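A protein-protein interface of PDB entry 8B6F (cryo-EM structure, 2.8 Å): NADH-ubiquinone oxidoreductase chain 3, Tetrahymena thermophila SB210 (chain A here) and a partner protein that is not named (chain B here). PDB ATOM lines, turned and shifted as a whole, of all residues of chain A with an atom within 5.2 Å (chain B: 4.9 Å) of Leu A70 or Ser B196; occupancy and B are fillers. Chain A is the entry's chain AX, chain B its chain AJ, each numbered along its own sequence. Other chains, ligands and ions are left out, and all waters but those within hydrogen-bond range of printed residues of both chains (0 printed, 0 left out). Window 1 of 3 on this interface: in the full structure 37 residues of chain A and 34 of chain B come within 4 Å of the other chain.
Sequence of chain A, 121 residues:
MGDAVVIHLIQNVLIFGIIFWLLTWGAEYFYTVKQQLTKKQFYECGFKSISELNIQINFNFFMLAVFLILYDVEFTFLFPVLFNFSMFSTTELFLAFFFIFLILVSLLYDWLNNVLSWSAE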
ATOM      1  N   VAL A  66      -1.869  -9.183   5.889  1.00  0.00           N
ATOM      2  CA  VAL A  66      -2.424  -8.854   7.199  1.00  0.00           C
ATOM      3  C   VAL A  66      -3.907  -8.537   7.078  1.00  0.00           C
ATOM      4  O   VAL A  66      -4.725  -9.001   7.880  1.00  0.00           O
ATOM      5  CB  VAL A  66      -1.641  -7.684   7.825  1.00  0.00           C
ATOM      6  CG1 VAL A  66      -2.426  -7.041   8.961  1.00  0.00           C
ATOM      7  CG2 VAL A  66      -0.288  -8.160   8.317  1.00  0.00           C
ATOM      8  N   PHE A  67      -4.274  -7.739   6.077  1.00  0.00           N
ATOM      9  CA  PHE A  67      -5.670  -7.367   5.893  1.00  0.00           C
ATOM     10  C   PHE A  67      -6.487  -8.513   5.321  1.00  0.00           C
ATOM     11  O   PHE A  67      -7.687  -8.614   5.599  1.00  0.00           O
ATOM     12  CB  PHE A  67      -5.766  -6.138   4.991  1.00  0.00           C
ATOM     13  CG  PHE A  67      -5.168  -4.898   5.593  1.00  0.00           C
ATOM     14  CD1 PHE A  67      -5.354  -4.598   6.932  1.00  0.00           C
ATOM     15  CD2 PHE A  67      -4.413  -4.037   4.819  1.00  0.00           C
ATOM     16  CE1 PHE A  67      -4.804  -3.463   7.485  1.00  0.00           C
ATOM     17  CE2 PHE A  67      -3.860  -2.903   5.365  1.00  0.00           C
ATOM     18  CZ  PHE A  67      -4.056  -2.613   6.701  1.00  0.00           C
ATOM     19  N   LEU A  68      -5.865  -9.385   4.528  1.00  0.00           N
ATOM     20  CA  LEU A  68      -6.581 -10.554   4.032  1.00  0.00           C
ATOM     21  C   LEU A  68      -7.006 -11.459   5.179  1.00  0.00           C
ATOM     22  O   LEU A  68      -8.108 -12.019   5.161  1.00  0.00           O
ATOM     23  CB  LEU A  68      -5.707 -11.323   3.043  1.00  0.00           C
ATOM     24  CG  LEU A  68      -6.348 -12.585   2.461  1.00  0.00           C
ATOM     25  CD1 LEU A  68      -7.511 -12.219   1.560  1.00  0.00           C
ATOM     26  CD2 LEU A  68      -5.329 -13.405   1.704  1.00  0.00           C
ATOM     27  N   ILE A  69      -6.143 -11.624   6.180  1.00  0.00           N
ATOM     28  CA  ILE A  69      -6.484 -12.470   7.319  1.00  0.00           C
ATOM     29  C   ILE A  69      -7.768 -11.981   7.977  1.00  0.00           C
ATOM     30  O   ILE A  69      -8.640 -12.778   8.341  1.00  0.00           O
ATOM     31  CB  ILE A  69      -5.314 -12.514   8.319  1.00  0.00           C
ATOM     32  CG1 ILE A  69      -4.108 -13.215   7.691  1.00  0.00           C
ATOM     33  CG2 ILE A  69      -5.724 -13.226   9.601  1.00  0.00           C
ATOM     34  CD1 ILE A  69      -2.818 -13.022   8.461  1.00  0.00           C
ATOM     35  N   LEU A  70      -7.906 -10.663   8.141  1.00  0.00           N
ATOM     36  CA  LEU A  70      -9.105 -10.122   8.774  1.00  0.00           C
ATOM     37  C   LEU A  70     -10.314 -10.206   7.851  1.00  0.00           C
ATOM     38  O   LEU A  70     -11.406 -10.589   8.284  1.00  0.00           O
ATOM     39  CB  LEU A  70      -8.862  -8.673   9.195  1.00  0.00           C
ATOM     40  CG  LEU A  70      -7.622  -8.410  10.051  1.00  0.00           C
ATOM     41  CD1 LEU A  70      -7.502  -6.930  10.373  1.00  0.00           C
ATOM     42  CD2 LEU A  70      -7.659  -9.232  11.326  1.00  0.00           C
ATOM     43  N   TYR A  71     -10.143  -9.847   6.577  1.00  0.00           N
ATOM     44  CA  TYR A  71     -11.293  -9.747   5.684  1.00  0.00           C
ATOM     45  C   TYR A  71     -11.836 -11.115   5.297  1.00  0.00           C
ATOM     46  O   TYR A  71     -13.022 -11.232   4.970  1.00  0.00           O
ATOM     47  CB  TYR A  71     -10.919  -8.942   4.442  1.00  0.00           C
ATOM     48  CG  TYR A  71     -10.495  -7.523   4.754  1.00  0.00           C
ATOM     49  CD1 TYR A  71     -10.932  -6.879   5.907  1.00  0.00           C
ATOM     50  CD2 TYR A  71      -9.652  -6.829   3.903  1.00  0.00           C
ATOM     51  CE1 TYR A  71     -10.546  -5.588   6.197  1.00  0.00           C
ATOM     52  CE2 TYR A  71      -9.259  -5.535   4.186  1.00  0.00           C
ATOM     53  CZ  TYR A  71      -9.710  -4.922   5.335  1.00  0.00           C
ATOM     54  OH  TYR A  71      -9.321  -3.635   5.620  1.00  0.00           O
ATOM     55  N   ASP A  72     -11.005 -12.157   5.326  1.00  0.00           N
ATOM     56  CA  ASP A  72     -11.522 -13.502   5.105  1.00  0.00           C
ATOM     57  C   ASP A  72     -12.541 -13.867   6.174  1.00  0.00           C
ATOM     58  O   ASP A  72     -13.613 -14.404   5.874  1.00  0.00           O
ATOM     59  CB  ASP A  72     -10.379 -14.517   5.088  1.00  0.00           C
ATOM     60  CG  ASP A  72      -9.648 -14.550   3.762  1.00  0.00           C
ATOM     61  OD1 ASP A  72     -10.052 -13.809   2.842  1.00  0.00           O
ATOM     62  OD2 ASP A  72      -8.673 -15.321   3.638  1.00  0.00           O
ATOM     63  N   VAL A  73     -12.219 -13.588   7.436  1.00  0.00           N
ATOM     64  CA  VAL A  73     -13.160 -13.868   8.513  1.00  0.00           C
ATOM     65  C   VAL A  73     -14.378 -12.960   8.412  1.00  0.00           C
ATOM     66  O   VAL A  73     -15.511 -13.391   8.650  1.00  0.00           O
ATOM     67  CB  VAL A  73     -12.481 -13.730   9.882  1.00  0.00           C
ATOM     68  CG1 VAL A  73     -13.446 -14.180  10.949  1.00  0.00           C
ATOM     69  CG2 VAL A  73     -11.190 -14.542   9.935  1.00  0.00           C
ATOM     70  N   GLU A  74     -14.168 -11.690   8.063  1.00  0.00           N
ATOM     71  CA  GLU A  74     -15.294 -10.774   7.920  1.00  0.00           C
ATOM     72  C   GLU A  74     -16.270 -11.279   6.869  1.00  0.00           C
ATOM     73  O   GLU A  74     -17.487 -11.261   7.081  1.00  0.00           O
ATOM     74  CB  GLU A  74     -14.792  -9.376   7.565  1.00  0.00           C
ATOM     75  CG  GLU A  74     -14.090  -8.672   8.713  1.00  0.00           C
ATOM     76  CD  GLU A  74     -13.642  -7.267   8.360  1.00  0.00           C
ATOM     77  OE1 GLU A  74     -13.649  -6.923   7.161  1.00  0.00           O
ATOM     78  OE2 GLU A  74     -13.285  -6.504   9.282  1.00  0.00           O
ATOM     79  N   PHE A  75     -15.755 -11.734   5.729  1.00  0.00           N
ATOM     80  CA  PHE A  75     -16.623 -12.284   4.696  1.00  0.00           C
ATOM     81  C   PHE A  75     -17.260 -13.590   5.153  1.00  0.00           C
ATOM     82  O   PHE A  75     -18.438 -13.843   4.872  1.00  0.00           O
ATOM     83  CB  PHE A  75     -15.829 -12.495   3.406  1.00  0.00           C
ATOM     84  CG  PHE A  75     -15.210 -11.238   2.861  1.00  0.00           C
ATOM     85  CD1 PHE A  75     -15.751  -9.992   3.145  1.00  0.00           C
ATOM     86  CD2 PHE A  75     -14.083 -11.303   2.057  1.00  0.00           C
ATOM     87  CE1 PHE A  75     -15.180  -8.840   2.642  1.00  0.00           C
ATOM     88  CE2 PHE A  75     -13.507 -10.154   1.552  1.00  0.00           C
ATOM     89  CZ  PHE A  75     -14.057  -8.921   1.844  1.00  0.00           C
ATOM     90  N   SER A 106     -13.382   0.090   7.277  1.00  0.00           N
ATOM     91  CA  SER A 106     -12.016  -0.387   7.456  1.00  0.00           C
ATOM     92  C   SER A 106     -11.235  -0.298   6.152  1.00  0.00           C
ATOM     93  O   SER A 106     -10.071   0.117   6.144  1.00  0.00           O
ATOM     94  CB  SER A 106     -12.023  -1.822   7.986  1.00  0.00           C
ATOM     95  OG  SER A 106     -12.644  -2.702   7.066  1.00  0.00           O
ATOM     96  N   TYR A 109     -10.354   3.338   5.554  1.00  0.00           N
ATOM     97  CA  TYR A 109      -9.243   3.775   6.393  1.00  0.00           C
ATOM     98  C   TYR A 109      -7.916   3.260   5.855  1.00  0.00           C
ATOM     99  O   TYR A 109      -6.918   3.987   5.843  1.00  0.00           O
ATOM    100  CB  TYR A 109      -9.455   3.311   7.832  1.00  0.00           C
ATOM    101  CG  TYR A 109      -8.364   3.759   8.776  1.00  0.00           C
ATOM    102  CD1 TYR A 109      -8.394   5.022   9.352  1.00  0.00           C
ATOM    103  CD2 TYR A 109      -7.307   2.918   9.092  1.00  0.00           C
ATOM    104  CE1 TYR A 109      -7.400   5.435  10.214  1.00  0.00           C
ATOM    105  CE2 TYR A 109      -6.309   3.323   9.954  1.00  0.00           C
ATOM    106  CZ  TYR A 109      -6.361   4.582  10.512  1.00  0.00           C
ATOM    107  OH  TYR A 109      -5.369   4.990  11.371  1.00  0.00           O
ATOM    108  N   ASP A 110      -7.882   2.003   5.408  1.00  0.00           N
ATOM    109  CA  ASP A 110      -6.663   1.472   4.809  1.00  0.00           C
ATOM    110  C   ASP A 110      -6.256   2.291   3.591  1.00  0.00           C
ATOM    111  O   ASP A 110      -5.078   2.627   3.426  1.00  0.00           O
ATOM    112  CB  ASP A 110      -6.866   0.006   4.426  1.00  0.00           C
ATOM    113  CG  ASP A 110      -7.203  -0.866   5.620  1.00  0.00           C
ATOM    114  OD1 ASP A 110      -6.761  -0.538   6.740  1.00  0.00           O
ATOM    115  OD2 ASP A 110      -7.908  -1.880   5.440  1.00  0.00           O
ATOM    116  N   LEU B 192     -12.599  -6.018  14.841  1.00  0.00           N
ATOM    117  CA  LEU B 192     -11.829  -6.129  13.608  1.00  0.00           C
ATOM    118  C   LEU B 192     -11.497  -4.756  13.037  1.00  0.00           C
ATOM    119  O   LEU B 192     -10.389  -4.542  12.533  1.00  0.00           O
ATOM    120  CB  LEU B 192     -12.594  -6.976  12.593  1.00  0.00           C
ATOM    121  CG  LEU B 192     -12.775  -8.443  12.999  1.00  0.00           C
ATOM    122  CD1 LEU B 192     -13.676  -9.167  12.022  1.00  0.00           C
ATOM    123  CD2 LEU B 192     -11.438  -9.159  13.099  1.00  0.00           C
ATOM    124  N   LEU B 193     -12.441  -3.814  13.096  1.00  0.00           N
ATOM    125  CA  LEU B 193     -12.153  -2.460  12.630  1.00  0.00           C
ATOM    126  C   LEU B 193     -11.032  -1.834  13.446  1.00  0.00           C
ATOM    127  O   LEU B 193     -10.076  -1.279  12.893  1.00  0.00           O
ATOM    128  CB  LEU B 193     -13.415  -1.601  12.705  1.00  0.00           C
ATOM    129  CG  LEU B 193     -13.240  -0.130  12.321  1.00  0.00           C
ATOM    130  CD1 LEU B 193     -12.807   0.015  10.873  1.00  0.00           C
ATOM    131  CD2 LEU B 193     -14.524   0.627  12.570  1.00  0.00           C
ATOM    132  N   LEU B 194     -11.138  -1.907  14.773  1.00  0.00           N
ATOM    133  CA  LEU B 194     -10.103  -1.347  15.631  1.00  0.00           C
ATOM    134  C   LEU B 194      -8.774  -2.060  15.425  1.00  0.00           C
ATOM    135  O   LEU B 194      -7.712  -1.438  15.517  1.00  0.00           O
ATOM    136  CB  LEU B 194     -10.533  -1.423  17.094  1.00  0.00           C
ATOM    137  CG  LEU B 194      -9.718  -0.586  18.082  1.00  0.00           C
ATOM    138  CD1 LEU B 194      -9.827   0.900  17.780  1.00  0.00           C
ATOM    139  CD2 LEU B 194     -10.173  -0.872  19.497  1.00  0.00           C
ATOM    140  N   GLY B 195      -8.818  -3.364  15.150  1.00  0.00           N
ATOM    141  CA  GLY B 195      -7.595  -4.098  14.874  1.00  0.00           C
ATOM    142  C   GLY B 195      -6.935  -3.665  13.580  1.00  0.00           C
ATOM    143  O   GLY B 195      -5.707  -3.589  13.496  1.00  0.00           O
ATOM    144  N   SER B 196      -7.734  -3.376  12.553  1.00  0.00           N
ATOM    145  CA  SER B 196      -7.170  -2.828  11.325  1.00  0.00           C
ATOM    146  C   SER B 196      -6.490  -1.492  11.592  1.00  0.00           C
ATOM    147  O   SER B 196      -5.387  -1.238  11.094  1.00  0.00           O
ATOM    148  CB  SER B 196      -8.264  -2.665  10.271  1.00  0.00           C
ATOM    149  OG  SER B 196      -8.884  -3.905   9.984  1.00  0.00           O
ATOM    150  N   VAL B 197      -7.129  -0.625  12.378  1.00  0.00           N
ATOM    151  CA  VAL B 197      -6.516   0.655  12.717  1.00  0.00           C
ATOM    152  C   VAL B 197      -5.205   0.426  13.457  1.00  0.00           C
ATOM    153  O   VAL B 197      -4.193   1.079  13.177  1.00  0.00           O
ATOM    154  CB  VAL B 197      -7.493   1.515  13.540  1.00  0.00           C
ATOM    155  CG1 VAL B 197      -6.826   2.803  14.006  1.00  0.00           C
ATOM    156  CG2 VAL B 197      -8.739   1.826  12.729  1.00  0.00           C
ATOM    157  N   ALA B 198      -5.204  -0.499  14.417  1.00  0.00           N
ATOM    158  CA  ALA B 198      -3.992  -0.776  15.180  1.00  0.00           C
ATOM    159  C   ALA B 198      -2.891  -1.328  14.286  1.00  0.00           C
ATOM    160  O   ALA B 198      -1.715  -0.987  14.453  1.00  0.00           O
ATOM    161  CB  ALA B 198      -4.297  -1.753  16.314  1.00  0.00           C
ATOM    162  N   CYS B 199      -3.252  -2.188  13.333  1.00  0.00           N
ATOM    163  CA  CYS B 199      -2.257  -2.719  12.408  1.00  0.00           C
ATOM    164  C   CYS B 199      -1.643  -1.612  11.560  1.00  0.00           C
ATOM    165  O   CYS B 199      -0.427  -1.588  11.347  1.00  0.00           O
ATOM    166  CB  CYS B 199      -2.893  -3.782  11.514  1.00  0.00           C
ATOM    167  SG  CYS B 199      -3.242  -5.345  12.350  1.00  0.00           S
ATOM    168  N   VAL B 200      -2.468  -0.687  11.067  1.00  0.00           N
ATOM    169  CA  VAL B 200      -1.944   0.431  10.288  1.00  0.00           C
ATOM    170  C   VAL B 200      -0.995   1.270  11.131  1.00  0.00           C
ATOM    171  O   VAL B 200       0.081   1.669  10.671  1.00  0.00           O
ATOM    172  CB  VAL B 200      -3.103   1.275   9.728  1.00  0.00           C
ATOM    173  CG1 VAL B 200      -2.584   2.556   9.090  1.00  0.00           C
ATOM    174  CG2 VAL B 200      -3.901   0.470   8.723  1.00  0.00           C
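Val A66 touches Cys B199 (CG1 to SG, 3.9 Å). Val B200 touches Phe A67. Ser B196 touches Leu A70 (OG to CD1, 3.3 Å). Glu A74 touches Leu B192 (CG to CD1, 3.4 Å). CB of Ser A106 touches CD1 of Leu B193, at 3.5 Å. Tyr A109 touches Val B197. Tyr A109 touches Val B200 (CE2 to CB, 3.8 Å). Asp A110 touches Val B200 (OD1 to CG2, 3.6 Å).
Of the 9 printed residues of chain B, 6 touch a printed residue of chain A. Hydrophobic or aromatic side chains of chain B within 4 Å of the printed part of chain A: Leu B192, Leu B193, Val B197 and Val B200. Of the 13 printed residues of chain A, 7 touch a printed residue of chain B. Among the printed residues, no Asp or Glu carboxylate lies within 4 Å of a Lys or Arg side-chain nitrogen of the other chain.
OG of Ser B196 lies within hydrogen-bond range of O of Leu B192 (3.0 Å). The backbone carbonyl oxygen (O) of Gly B195 is in hydrogen-bond range of the side-chain sulfur (SG) of Cys B199.
Leu A68 touches none of the printed residues of chain B. Leu A70 touches one residue of chain B. Of the printed residues of chain B, Glu A74 touches Leu B192 (3.4 Å). Printed residues of chain B within 4 Å of Tyr A109: Val B197 and Val B200. Of the printed residues of chain B, Asp A110 touches Val B200 (3.6 Å). Ser B196 touches just one residue of chain A: Leu A70 (3.3 Å). Printed residues of chain A within 4 Å of Val B197: Tyr A109 (3.7 Å). The nearest printed residue of chain A that does not touch Val B197 is Asp A110 (5.7 Å).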
